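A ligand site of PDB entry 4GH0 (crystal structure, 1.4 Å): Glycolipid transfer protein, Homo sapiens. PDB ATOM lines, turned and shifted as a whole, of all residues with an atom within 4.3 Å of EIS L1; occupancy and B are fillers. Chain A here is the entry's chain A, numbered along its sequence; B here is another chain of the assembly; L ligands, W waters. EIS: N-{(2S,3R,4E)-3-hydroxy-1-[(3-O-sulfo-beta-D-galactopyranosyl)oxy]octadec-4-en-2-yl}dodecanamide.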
ATOM      1  N   PHE A  34      -4.063  17.506  12.096  1.00  0.00           N
ATOM      2  CA  PHE A  34      -5.039  17.719  11.045  1.00  0.00           C
ATOM      3  C   PHE A  34      -5.199  19.211  10.654  1.00  0.00           C
ATOM      4  O   PHE A  34      -5.626  19.514   9.533  1.00  0.00           O
ATOM      5  CB  PHE A  34      -6.360  17.076  11.431  1.00  0.00           C
ATOM      6  CG  PHE A  34      -6.324  15.578  11.310  1.00  0.00           C
ATOM      7  CD1 PHE A  34      -6.710  14.943  10.146  1.00  0.00           C
ATOM      8  CD2 PHE A  34      -5.825  14.809  12.350  1.00  0.00           C
ATOM      9  CE1 PHE A  34      -6.651  13.551  10.018  1.00  0.00           C
ATOM     10  CE2 PHE A  34      -5.734  13.424  12.237  1.00  0.00           C
ATOM     11  CZ  PHE A  34      -6.152  12.804  11.076  1.00  0.00           C
ATOM     12  N   VAL A  41     -11.112  21.121   5.106  1.00  0.00           N
ATOM     13  CA  VAL A  41     -11.827  19.894   4.862  1.00  0.00           C
ATOM     14  C   VAL A  41     -11.561  18.868   5.981  1.00  0.00           C
ATOM     15  O   VAL A  41     -12.411  18.025   6.296  1.00  0.00           O
ATOM     16  CB  VAL A  41     -11.435  19.292   3.471  1.00  0.00           C
ATOM     17  CG1 VAL A  41     -11.739  17.828   3.374  1.00  0.00           C
ATOM     18  CG2 VAL A  41     -12.119  20.062   2.365  1.00  0.00           C
ATOM     19  N   PHE A  42     -10.374  18.931   6.588  1.00  0.00           N
ATOM     20  CA  PHE A  42      -9.981  17.978   7.617  1.00  0.00           C
ATOM     21  C   PHE A  42     -10.388  18.353   9.010  1.00  0.00           C
ATOM     22  O   PHE A  42     -10.260  17.535   9.927  1.00  0.00           O
ATOM     23  CB  PHE A  42      -8.498  17.665   7.468  1.00  0.00           C
ATOM     24  CG  PHE A  42      -8.159  17.208   6.085  1.00  0.00           C
ATOM     25  CD1 PHE A  42      -8.746  16.056   5.569  1.00  0.00           C
ATOM     26  CD2 PHE A  42      -7.372  17.973   5.250  1.00  0.00           C
ATOM     27  CE1 PHE A  42      -8.498  15.634   4.286  1.00  0.00           C
ATOM     28  CE2 PHE A  42      -7.126  17.561   3.966  1.00  0.00           C
ATOM     29  CZ  PHE A  42      -7.697  16.394   3.469  1.00  0.00           C
ATOM     30  N   PRO A  44     -13.523  18.507  10.312  1.00  0.00           N
ATOM     31  CA  PRO A  44     -14.463  17.556  10.909  1.00  0.00           C
ATOM     32  C   PRO A  44     -13.828  16.207  11.274  1.00  0.00           C
ATOM     33  O   PRO A  44     -14.296  15.552  12.223  1.00  0.00           O
ATOM     34  CB  PRO A  44     -15.579  17.439   9.871  1.00  0.00           C
ATOM     35  CG  PRO A  44     -15.437  18.666   8.994  1.00  0.00           C
ATOM     36  CD  PRO A  44     -13.955  18.916   8.953  1.00  0.00           C
ATOM     37  N   ILE A  45     -12.780  15.808  10.577  1.00  0.00           N
ATOM     38  CA  ILE A  45     -12.054  14.587  10.933  1.00  0.00           C
ATOM     39  C   ILE A  45     -11.315  14.768  12.240  1.00  0.00           C
ATOM     40  O   ILE A  45     -11.399  13.900  13.132  1.00  0.00           O
ATOM     41  CB  ILE A  45     -11.098  14.146   9.817  1.00  0.00           C
ATOM     42  CG1 ILE A  45     -11.891  13.937   8.531  1.00  0.00           C
ATOM     43  CG2 ILE A  45     -10.405  12.863  10.226  1.00  0.00           C
ATOM     44  CD1 ILE A  45     -13.133  13.090   8.699  1.00  0.00           C
ATOM     45  N   GLY A  51     -13.258  13.597  19.530  1.00  0.00           N
ATOM     46  CA  GLY A  51     -14.409  13.083  20.262  1.00  0.00           C
ATOM     47  C   GLY A  51     -14.180  11.702  20.811  1.00  0.00           C
ATOM     48  O   GLY A  51     -14.592  11.383  21.931  1.00  0.00           O
ATOM     49  N   ASN A  52     -13.573  10.827  20.027  1.00  0.00           N
ATOM     50  CA  ASN A  52     -13.244   9.501  20.544  1.00  0.00           C
ATOM     51  C   ASN A  52     -12.332   9.591  21.758  1.00  0.00           C
ATOM     52  O   ASN A  52     -12.530   8.920  22.772  1.00  0.00           O
ATOM     53  CB  ASN A  52     -12.475   8.649  19.520  1.00  0.00           C
ATOM     54  CG  ASN A  52     -13.227   8.325  18.244  1.00  0.00           C
ATOM     55  OD1 ASN A  52     -12.604   8.230  17.190  1.00  0.00           O
ATOM     56  ND2 ASN A  52     -14.520   8.093  18.326  1.00  0.00           N
ATOM     57  N   LEU A  92     -16.456   1.358  22.518  1.00  0.00           N
ATOM     58  CA  LEU A  92     -16.847   1.798  21.190  1.00  0.00           C
ATOM     59  C   LEU A  92     -15.975   2.940  20.679  1.00  0.00           C
ATOM     60  O   LEU A  92     -15.562   2.972  19.536  1.00  0.00           O
ATOM     61  CB  LEU A  92     -18.339   2.171  21.149  1.00  0.00           C
ATOM     62  CG  LEU A  92     -18.913   2.599  19.818  1.00  0.00           C
ATOM     63  CD1 LEU A  92     -18.799   1.498  18.808  1.00  0.00           C
ATOM     64  CD2 LEU A  92     -20.384   3.050  19.987  1.00  0.00           C
ATOM     65  N   ALA A  93     -15.679   3.893  21.539  1.00  0.00           N
ATOM     66  CA  ALA A  93     -14.844   5.023  21.167  1.00  0.00           C
ATOM     67  C   ALA A  93     -13.464   4.549  20.739  1.00  0.00           C
ATOM     68  O   ALA A  93     -12.913   5.030  19.750  1.00  0.00           O
ATOM     69  CB  ALA A  93     -14.750   6.041  22.301  1.00  0.00           C
ATOM     70  N   TRP A  96     -13.330   2.831  17.302  1.00  0.00           N
ATOM     71  CA  TRP A  96     -13.219   3.752  16.185  1.00  0.00           C
ATOM     72  C   TRP A  96     -11.884   4.477  16.153  1.00  0.00           C
ATOM     73  O   TRP A  96     -11.316   4.707  15.083  1.00  0.00           O
ATOM     74  CB  TRP A  96     -14.410   4.703  16.176  1.00  0.00           C
ATOM     75  CG  TRP A  96     -15.657   4.004  15.642  1.00  0.00           C
ATOM     76  CD1 TRP A  96     -16.695   3.468  16.360  1.00  0.00           C
ATOM     77  CD2 TRP A  96     -15.929   3.725  14.271  1.00  0.00           C
ATOM     78  NE1 TRP A  96     -17.606   2.906  15.505  1.00  0.00           N
ATOM     79  CE2 TRP A  96     -17.167   3.069  14.209  1.00  0.00           C
ATOM     80  CE3 TRP A  96     -15.260   4.009  13.058  1.00  0.00           C
ATOM     81  CZ2 TRP A  96     -17.733   2.635  13.023  1.00  0.00           C
ATOM     82  CZ3 TRP A  96     -15.826   3.587  11.880  1.00  0.00           C
ATOM     83  CH2 TRP A  96     -17.077   2.933  11.871  1.00  0.00           C
ATOM     84  N   GLY A 100      -8.824   4.854  13.089  1.00  0.00           N
ATOM     85  CA  GLY A 100      -8.113   6.058  12.664  1.00  0.00           C
ATOM     86  C   GLY A 100      -6.598   5.961  12.859  1.00  0.00           C
ATOM     87  O   GLY A 100      -5.822   6.385  11.999  1.00  0.00           O
ATOM     88  N   PHE A 103      -5.329   3.744  10.102  1.00  0.00           N
ATOM     89  CA  PHE A 103      -5.231   4.496   8.867  1.00  0.00           C
ATOM     90  C   PHE A 103      -3.924   5.255   8.824  1.00  0.00           C
ATOM     91  O   PHE A 103      -3.206   5.231   7.797  1.00  0.00           O
ATOM     92  CB  PHE A 103      -6.432   5.463   8.745  1.00  0.00           C
ATOM     93  CG  PHE A 103      -6.414   6.335   7.515  1.00  0.00           C
ATOM     94  CD1 PHE A 103      -7.121   5.966   6.412  1.00  0.00           C
ATOM     95  CD2 PHE A 103      -5.632   7.480   7.465  1.00  0.00           C
ATOM     96  CE1 PHE A 103      -7.085   6.747   5.263  1.00  0.00           C
ATOM     97  CE2 PHE A 103      -5.566   8.221   6.276  1.00  0.00           C
ATOM     98  CZ  PHE A 103      -6.296   7.842   5.208  1.00  0.00           C
ATOM     99  N   LEU A 136     -10.430   1.448   7.018  1.00  0.00           N
ATOM    100  CA  LEU A 136     -11.769   2.035   7.191  1.00  0.00           C
ATOM    101  C   LEU A 136     -12.855   1.575   6.245  1.00  0.00           C
ATOM    102  O   LEU A 136     -14.019   1.541   6.619  1.00  0.00           O
ATOM    103  CB  LEU A 136     -11.664   3.566   7.012  1.00  0.00           C
ATOM    104  CG  LEU A 136     -10.910   4.330   8.107  1.00  0.00           C
ATOM    105  CD1 LEU A 136     -10.704   5.775   7.711  1.00  0.00           C
ATOM    106  CD2 LEU A 136     -11.666   4.234   9.409  1.00  0.00           C
ATOM    107  N   HIS A 140     -17.654   1.454   5.956  1.00  0.00           N
ATOM    108  CA  HIS A 140     -18.271   2.614   5.328  1.00  0.00           C
ATOM    109  C   HIS A 140     -19.172   2.207   4.186  1.00  0.00           C
ATOM    110  O   HIS A 140     -18.774   1.485   3.278  1.00  0.00           O
ATOM    111  CB  HIS A 140     -17.178   3.546   4.773  1.00  0.00           C
ATOM    112  CG  HIS A 140     -16.467   4.338   5.819  1.00  0.00           C
ATOM    113  ND1 HIS A 140     -15.405   5.148   5.519  1.00  0.00           N
ATOM    114  CD2 HIS A 140     -16.639   4.411   7.158  1.00  0.00           C
ATOM    115  CE1 HIS A 140     -14.981   5.742   6.622  1.00  0.00           C
ATOM    116  NE2 HIS A 140     -15.697   5.295   7.640  1.00  0.00           N
ATOM    117  N   VAL A 144     -20.427   7.550   2.387  1.00  0.00           N
ATOM    118  CA  VAL A 144     -19.224   7.884   3.108  1.00  0.00           C
ATOM    119  C   VAL A 144     -18.000   7.659   2.221  1.00  0.00           C
ATOM    120  O   VAL A 144     -17.066   8.466   2.194  1.00  0.00           O
ATOM    121  CB  VAL A 144     -19.131   7.136   4.448  1.00  0.00           C
ATOM    122  CG1 VAL A 144     -17.779   7.378   5.110  1.00  0.00           C
ATOM    123  CG2 VAL A 144     -20.268   7.554   5.369  1.00  0.00           C
ATOM    124  N   ILE A 147     -17.704  10.568  -0.075  1.00  0.00           N
ATOM    125  CA  ILE A 147     -17.146  11.741   0.596  1.00  0.00           C
ATOM    126  C   ILE A 147     -15.639  11.611   0.776  1.00  0.00           C
ATOM    127  O   ILE A 147     -14.917  12.574   0.554  1.00  0.00           O
ATOM    128  CB  ILE A 147     -17.846  12.003   1.903  1.00  0.00           C
ATOM    129  CG1 ILE A 147     -19.286  12.430   1.613  1.00  0.00           C
ATOM    130  CG2 ILE A 147     -17.138  13.086   2.717  1.00  0.00           C
ATOM    131  CD1 ILE A 147     -20.146  12.415   2.797  1.00  0.00           C
ATOM    132  N   PHE A 148     -15.130  10.447   1.175  1.00  0.00           N
ATOM    133  CA  PHE A 148     -13.685  10.217   1.194  1.00  0.00           C
ATOM    134  C   PHE A 148     -13.057  10.549  -0.163  1.00  0.00           C
ATOM    135  O   PHE A 148     -12.026  11.239  -0.208  1.00  0.00           O
ATOM    136  CB  PHE A 148     -13.345   8.757   1.585  1.00  0.00           C
ATOM    137  CG  PHE A 148     -11.886   8.391   1.365  1.00  0.00           C
ATOM    138  CD1 PHE A 148     -10.921   8.820   2.230  1.00  0.00           C
ATOM    139  CD2 PHE A 148     -11.494   7.674   0.234  1.00  0.00           C
ATOM    140  CE1 PHE A 148      -9.573   8.505   2.009  1.00  0.00           C
ATOM    141  CE2 PHE A 148     -10.156   7.369   0.023  1.00  0.00           C
ATOM    142  CZ  PHE A 148      -9.218   7.807   0.921  1.00  0.00           C
ATOM    143  N   ALA A 151     -12.897  14.215  -0.727  1.00  0.00           N
ATOM    144  CA  ALA A 151     -11.931  14.824   0.196  1.00  0.00           C
ATOM    145  C   ALA A 151     -10.496  14.694  -0.256  1.00  0.00           C
ATOM    146  O   ALA A 151      -9.679  15.533   0.107  1.00  0.00           O
ATOM    147  CB  ALA A 151     -12.089  14.221   1.583  1.00  0.00           C
ATOM    148  N   TYR A 207     -20.404  -3.469  11.712  1.00  0.00           N
ATOM    149  CA  TYR A 207     -21.442  -2.667  11.111  1.00  0.00           C
ATOM    150  C   TYR A 207     -20.848  -1.551  10.256  1.00  0.00           C
ATOM    151  O   TYR A 207     -19.724  -1.090  10.492  1.00  0.00           O
ATOM    152  CB  TYR A 207     -22.423  -2.136  12.157  1.00  0.00           C
ATOM    153  CG  TYR A 207     -21.855  -1.086  13.087  1.00  0.00           C
ATOM    154  CD1 TYR A 207     -21.986   0.257  12.784  1.00  0.00           C
ATOM    155  CD2 TYR A 207     -21.246  -1.443  14.261  1.00  0.00           C
ATOM    156  CE1 TYR A 207     -21.461   1.251  13.646  1.00  0.00           C
ATOM    157  CE2 TYR A 207     -20.724  -0.467  15.147  1.00  0.00           C
ATOM    158  CZ  TYR A 207     -20.848   0.876  14.832  1.00  0.00           C
ATOM    159  OH  TYR A 207     -20.346   1.863  15.668  1.00  0.00           O
ATOM    160  N   VAL A 209     -21.287   2.335   8.566  1.00  0.00           N
ATOM    161  CA  VAL A 209     -21.891   3.645   8.731  1.00  0.00           C
ATOM    162  C   VAL A 209     -22.176   4.307   7.389  1.00  0.00           C
ATOM    163  O   VAL A 209     -21.464   4.224   6.392  1.00  0.00           O
ATOM    164  CB  VAL A 209     -21.021   4.560   9.616  1.00  0.00           C
ATOM    165  CG1 VAL A 209     -20.873   3.982  11.017  1.00  0.00           C
ATOM    166  CG2 VAL A 209     -19.675   4.816   9.003  1.00  0.00           C
ATOM    167  N   PRO B  40     -24.856   8.359   9.786  1.00  0.00           N
ATOM    168  CA  PRO B  40     -23.512   8.634  10.302  1.00  0.00           C
ATOM    169  C   PRO B  40     -22.691   9.675   9.506  1.00  0.00           C
ATOM    170  O   PRO B  40     -21.695  10.183  10.009  1.00  0.00           O
ATOM    171  CB  PRO B  40     -22.842   7.265  10.236  1.00  0.00           C
ATOM    172  CG  PRO B  40     -23.984   6.265  10.237  1.00  0.00           C
ATOM    173  CD  PRO B  40     -25.119   6.910   9.579  1.00  0.00           C
ATOM    174  N   THR B  43     -22.184  12.660  11.714  1.00  0.00           N
ATOM    175  CA  THR B  43     -21.317  12.616  12.891  1.00  0.00           C
ATOM    176  C   THR B  43     -20.199  13.655  12.909  1.00  0.00           C
ATOM    177  O   THR B  43     -19.987  14.296  13.954  1.00  0.00           O
ATOM    178  CB  THR B  43     -20.771  11.190  13.075  1.00  0.00           C
ATOM    179  OG1 THR B  43     -21.908  10.366  13.276  1.00  0.00           O
ATOM    180  CG2 THR B  43     -19.833  11.087  14.249  1.00  0.00           C
ATOM    181  N   PRO B  44     -19.476  13.825  11.785  1.00  0.00           N
ATOM    182  CA  PRO B  44     -18.444  14.863  11.835  1.00  0.00           C
ATOM    183  C   PRO B  44     -19.003  16.272  12.001  1.00  0.00           C
ATOM    184  O   PRO B  44     -18.319  17.142  12.583  1.00  0.00           O
ATOM    185  CB  PRO B  44     -17.661  14.668  10.538  1.00  0.00           C
ATOM    186  CG  PRO B  44     -17.992  13.261  10.080  1.00  0.00           C
ATOM    187  CD  PRO B  44     -19.419  13.064  10.513  1.00  0.00           C
ATOM    188  N   VAL B 144     -15.414  22.110  -0.273  1.00  0.00           N
ATOM    189  CA  VAL B 144     -16.361  22.018   0.811  1.00  0.00           C
ATOM    190  C   VAL B 144     -17.787  22.042   0.267  1.00  0.00           C
ATOM    191  O   VAL B 144     -18.663  21.300   0.705  1.00  0.00           O
ATOM    192  CB  VAL B 144     -16.110  23.088   1.886  1.00  0.00           C
ATOM    193  CG1 VAL B 144     -17.219  23.075   2.932  1.00  0.00           C
ATOM    194  CG2 VAL B 144     -14.750  22.880   2.535  1.00  0.00           C
ATOM    195  N   ILE B 147     -18.596  18.662  -1.030  1.00  0.00           N
ATOM    196  CA  ILE B 147     -18.905  17.722   0.046  1.00  0.00           C
ATOM    197  C   ILE B 147     -20.318  17.948   0.594  1.00  0.00           C
ATOM    198  O   ILE B 147     -21.028  16.989   0.833  1.00  0.00           O
ATOM    199  CB  ILE B 147     -17.864  17.780   1.133  1.00  0.00           C
ATOM    200  CG1 ILE B 147     -16.543  17.231   0.581  1.00  0.00           C
ATOM    201  CG2 ILE B 147     -18.282  16.970   2.361  1.00  0.00           C
ATOM    202  CD1 ILE B 147     -15.394  17.528   1.437  1.00  0.00           C
HETATM  203  C43 EIS L   1     -18.295   6.884  15.265  1.00  0.00           C
HETATM  204  O   EIS L   1     -18.020   7.506  14.042  1.00  0.00           O
HETATM  205  C44 EIS L   1     -18.129   7.883  16.381  1.00  0.00           C
HETATM  206  O3  EIS L   1     -16.787   8.320  16.418  1.00  0.00           O
HETATM  207  C45 EIS L   1     -18.462   7.187  17.673  1.00  0.00           C
HETATM  208  C46 EIS L   1     -19.853   6.569  17.658  1.00  0.00           C
HETATM  209  O5  EIS L   1     -20.818   7.607  17.606  1.00  0.00           O
HETATM  210  C47 EIS L   1     -20.004   5.696  16.441  1.00  0.00           C
HETATM  211  C48 EIS L   1     -21.438   5.206  16.354  1.00  0.00           C
HETATM  212  O7  EIS L   1     -21.447   4.225  15.335  1.00  0.00           O
HETATM  213  O6  EIS L   1     -19.649   6.438  15.263  1.00  0.00           O
HETATM  214  O1  EIS L   1     -19.499   8.285  11.224  1.00  0.00           O
HETATM  215  C2  EIS L   1     -18.104   8.567  11.437  1.00  0.00           C
HETATM  216  C1  EIS L   1     -17.431   7.204  11.706  1.00  0.00           C
HETATM  217  N   EIS L   1     -15.998   7.339  12.004  1.00  0.00           N
HETATM  218  C   EIS L   1     -18.069   6.561  12.943  1.00  0.00           C
HETATM  219  C3  EIS L   1     -17.417   9.226  10.262  1.00  0.00           C
HETATM  220  C4  EIS L   1     -18.005   9.382   9.082  1.00  0.00           C
HETATM  221  C5  EIS L   1     -17.272  10.019   7.915  1.00  0.00           C
HETATM  222  C6  EIS L   1     -15.786   9.640   7.907  1.00  0.00           C
HETATM  223  C7  EIS L   1     -15.190   9.383   6.532  1.00  0.00           C
HETATM  224  C8  EIS L   1     -15.331  10.573   5.588  1.00  0.00           C
HETATM  225  C9  EIS L   1     -14.097  11.481   5.617  1.00  0.00           C
HETATM  226  C10 EIS L   1     -14.551  12.928   5.580  1.00  0.00           C
HETATM  227  C11 EIS L   1     -13.433  13.883   5.201  1.00  0.00           C
HETATM  228  C12 EIS L   1     -13.948  15.277   4.864  1.00  0.00           C
HETATM  229  C13 EIS L   1     -15.215  15.695   5.620  1.00  0.00           C
HETATM  230  C14 EIS L   1     -15.410  17.157   5.483  1.00  0.00           C
HETATM  231  C15 EIS L   1     -15.325  18.351   5.046  1.00  0.00           C
HETATM  232  C16 EIS L   1     -15.226  19.511   4.093  1.00  0.00           C
HETATM  233  C17 EIS L   1     -16.581  19.774   3.466  1.00  0.00           C
HETATM  234  C29 EIS L   1      -8.658  11.993   3.186  1.00  0.00           C
HETATM  235  C28 EIS L   1      -7.806  11.705   4.407  1.00  0.00           C
HETATM  236  C27 EIS L   1      -8.582  10.848   5.407  1.00  0.00           C
HETATM  237  C26 EIS L   1      -7.997  10.880   6.817  1.00  0.00           C
HETATM  238  C25 EIS L   1      -8.819   9.918   7.684  1.00  0.00           C
HETATM  239  C24 EIS L   1      -8.376   9.909   9.130  1.00  0.00           C
HETATM  240  C23 EIS L   1      -9.072   8.822   9.955  1.00  0.00           C
HETATM  241  C22 EIS L   1     -10.591   8.930   9.871  1.00  0.00           C
HETATM  242  C21 EIS L   1     -11.319   8.052  10.887  1.00  0.00           C
HETATM  243  C20 EIS L   1     -12.798   7.943  10.521  1.00  0.00           C
HETATM  244  C19 EIS L   1     -13.586   7.105  11.530  1.00  0.00           C
HETATM  245  C18 EIS L   1     -15.038   6.975  11.122  1.00  0.00           C
HETATM  246  O2  EIS L   1     -15.326   6.510  10.033  1.00  0.00           O
HETATM  247  S   EIS L   1     -17.810   7.705  20.160  1.00  0.00           S
HETATM  248  O4  EIS L   1     -18.313   8.143  18.706  1.00  0.00           O
HETATM  249  O10 EIS L   1     -18.009   6.290  20.439  1.00  0.00           O
HETATM  250  O9  EIS L   1     -16.371   8.009  20.221  1.00  0.00           O
HETATM  251  O8  EIS L   1     -18.563   8.562  21.100  1.00  0.00           O
HETATM  252  C43 EIS L   2     -13.960  26.149  12.073  1.00  0.00           C
HETATM  253  O   EIS L   2     -14.536  25.244  11.175  1.00  0.00           O
HETATM  254  C44 EIS L   2     -13.777  25.478  13.410  1.00  0.00           C
HETATM  255  O3  EIS L   2     -15.040  25.114  13.923  1.00  0.00           O
HETATM  256  C45 EIS L   2     -13.128  26.471  14.336  1.00  0.00           C
HETATM  257  C46 EIS L   2     -11.818  27.012  13.782  1.00  0.00           C
HETATM  258  O5  EIS L   2     -10.867  25.961  13.736  1.00  0.00           O
HETATM  259  C47 EIS L   2     -12.038  27.537  12.388  1.00  0.00           C
HETATM  260  C48 EIS L   2     -10.702  27.935  11.788  1.00  0.00           C
HETATM  261  O7  EIS L   2     -11.008  28.618  10.589  1.00  0.00           O
HETATM  262  O6  EIS L   2     -12.675  26.529  11.584  1.00  0.00           O
HETATM  263  O1  EIS L   2     -13.858  23.711   8.360  1.00  0.00           O
HETATM  264  C2  EIS L   2     -15.130  23.545   9.011  1.00  0.00           C
HETATM  265  C1  EIS L   2     -15.753  24.954   9.095  1.00  0.00           C
HETATM  266  N   EIS L   2     -17.042  24.944   9.799  1.00  0.00           N
HETATM  267  C   EIS L   2     -14.825  25.871   9.900  1.00  0.00           C
HETATM  268  C3  EIS L   2     -16.088  22.631   8.281  1.00  0.00           C
HETATM  269  C4  EIS L   2     -15.841  22.155   7.067  1.00  0.00           C
HETATM  270  C5  EIS L   2     -16.841  21.266   6.350  1.00  0.00           C
HETATM  271  C6  EIS L   2     -18.285  21.684   6.652  1.00  0.00           C
HETATM  272  C7  EIS L   2     -19.244  21.600   5.475  1.00  0.00           C
HETATM  273  C8  EIS L   2     -19.324  20.203   4.868  1.00  0.00           C
HETATM  274  C9  EIS L   2     -20.469  19.379   5.467  1.00  0.00           C
HETATM  275  C10 EIS L   2     -19.989  17.955   5.681  1.00  0.00           C
HETATM  276  C11 EIS L   2     -21.133  16.976   5.883  1.00  0.00           C
HETATM  277  C12 EIS L   2     -20.679  15.525   5.788  1.00  0.00           C
HETATM  278  C13 EIS L   2     -19.239  15.270   6.249  1.00  0.00           C
HETATM  279  C14 EIS L   2     -19.035  13.816   6.445  1.00  0.00           C
HETATM  280  C15 EIS L   2     -19.192  12.544   6.373  1.00  0.00           C
HETATM  281  C16 EIS L   2     -19.507  11.191   5.814  1.00  0.00           C
HETATM  282  C17 EIS L   2     -18.367  10.726   4.929  1.00  0.00           C
HETATM  283  C29 EIS L   2     -26.344  18.457   4.837  1.00  0.00           C
HETATM  284  C28 EIS L   2     -26.838  19.081   6.128  1.00  0.00           C
HETATM  285  C27 EIS L   2     -25.848  20.128   6.621  1.00  0.00           C
HETATM  286  C26 EIS L   2     -26.024  20.491   8.095  1.00  0.00           C
HETATM  287  C25 EIS L   2     -25.032  21.613   8.426  1.00  0.00           C
HETATM  288  C24 EIS L   2     -25.072  22.010   9.886  1.00  0.00           C
HETATM  289  C23 EIS L   2     -24.207  23.248  10.179  1.00  0.00           C
HETATM  290  C22 EIS L   2     -22.766  23.066   9.713  1.00  0.00           C
HETATM  291  C21 EIS L   2     -21.820  24.149  10.228  1.00  0.00           C
HETATM  292  C20 EIS L   2     -20.503  24.106   9.456  1.00  0.00           C
HETATM  293  C19 EIS L   2     -19.500  25.146   9.958  1.00  0.00           C
HETATM  294  C18 EIS L   2     -18.222  25.113   9.149  1.00  0.00           C
HETATM  295  O2  EIS L   2     -18.260  25.271   7.942  1.00  0.00           O
HETATM  296  S   EIS L   2     -13.054  26.634  16.953  1.00  0.00           S
HETATM  297  O4  EIS L   2     -12.953  25.819  15.580  1.00  0.00           O
HETATM  298  O10 EIS L   2     -12.838  28.065  16.792  1.00  0.00           O
HETATM  299  O9  EIS L   2     -14.409  26.409  17.481  1.00  0.00           O
HETATM  300  O8  EIS L   2     -12.042  26.022  17.838  1.00  0.00           O
HETATM  301  O   HOH W   1     -12.285   7.586  14.683  1.00  0.00           O
HETATM  302  O   HOH W   2     -21.413   7.769  13.379  1.00  0.00           O
HETATM  303  O   HOH W   3     -23.932   3.976  14.387  1.00  0.00           O
HETATM  304  O   HOH W   4     -14.763   7.873  14.620  1.00  0.00           O
HETATM  305  O   HOH W   5     -17.235  11.251  19.880  1.00  0.00           O
HETATM  306  O   HOH W   6     -20.372  10.776  17.924  1.00  0.00           O
HETATM  307  O   HOH W   7     -16.401  10.829  17.352  1.00  0.00           O
HETATM  308  O   HOH W   8     -19.194   5.463  22.858  1.00  0.00           O
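Residues that only touch EIS L1: Val 41 (3.2 Å), Ile 147 of chain B (3.3 Å), Ala 93 (3.3 Å), Val 144 of chain B (3.4 Å), Ile 45 (3.4 Å), Trp 96 (3.5 Å), Val 144 of chain A (3.6 Å), Phe 103 (3.6 Å), Thr 43 of chain B (3.7 Å), Phe 148 (3.8 Å), Phe 42 (3.8 Å), Pro 44 of chain A (3.8 Å), Leu 136 (3.8 Å), Leu 92 (3.9 Å), Ile 147 of chain A (3.9 Å), Ala 151 (3.9 Å), Pro 44 of chain B (3.96 Å) and Gly 100 (3.99 Å). Within 4 Å of EIS L1: Val 41, Phe 42, Pro 44 of chain A, Ile 45, Asn 52, Leu 92, Ala 93, Trp 96, Gly 100, Phe 103, Leu 136, His 140, Val 144 of chain A, Ile 147 of chain A, Phe 148, Ala 151, Tyr 207, Pro 40 of chain B, Thr 43 of chain B, Pro 44 of chain B, Val 144 of chain B and Ile 147 of chain B.
Water W7 lies within hydrogen-bond range of O3 of EIS L1 (2.7 Å) and ND2 of Asn 52 (3.5 Å). Water W4 lies within hydrogen-bond range of an oxygen (O3) of EIS L1 (2.7 Å) and the side-chain amide oxygen (OD1) of Asn 52 (3.4 Å). Water W2 lies within hydrogen-bond range of OG1 of Thr 43 of chain B (2.6 Å) and O6 of EIS L1 (2.9 Å). Water W5 bridges O8 of EIS L1 and O of Gly 51. Water W1 bridges the side-chain amide oxygen (OD1) of Asn 52 and the backbone carbonyl oxygen (O) of Trp 96.
The side-chain hydroxyl (OH) of Tyr 207 is in hydrogen-bond range of an oxygen (O7) of EIS L1 (2.6 Å). The side-chain amide nitrogen (ND2) of Asn 52 lies within hydrogen-bond range of an oxygen (O9) of EIS L1. An oxygen (O2) of EIS L1 is in hydrogen-bond range of a ring nitrogen (NE2) of His 140, at 2.7 Å. The backbone carbonyl oxygen of Pro 40 of chain B sits at hydrogen-bond distance from an oxygen (O1) of EIS L1 (3.1 Å).
NE1 of Trp 96 is in hydrogen-bond range of OH of Tyr 207 (2.9 Å). The side-chain hydroxyl (OG1) of Thr 43 of chain B is in hydrogen-bond range of the backbone carbonyl oxygen (O) of Pro 40 of chain B (3.3 Å).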
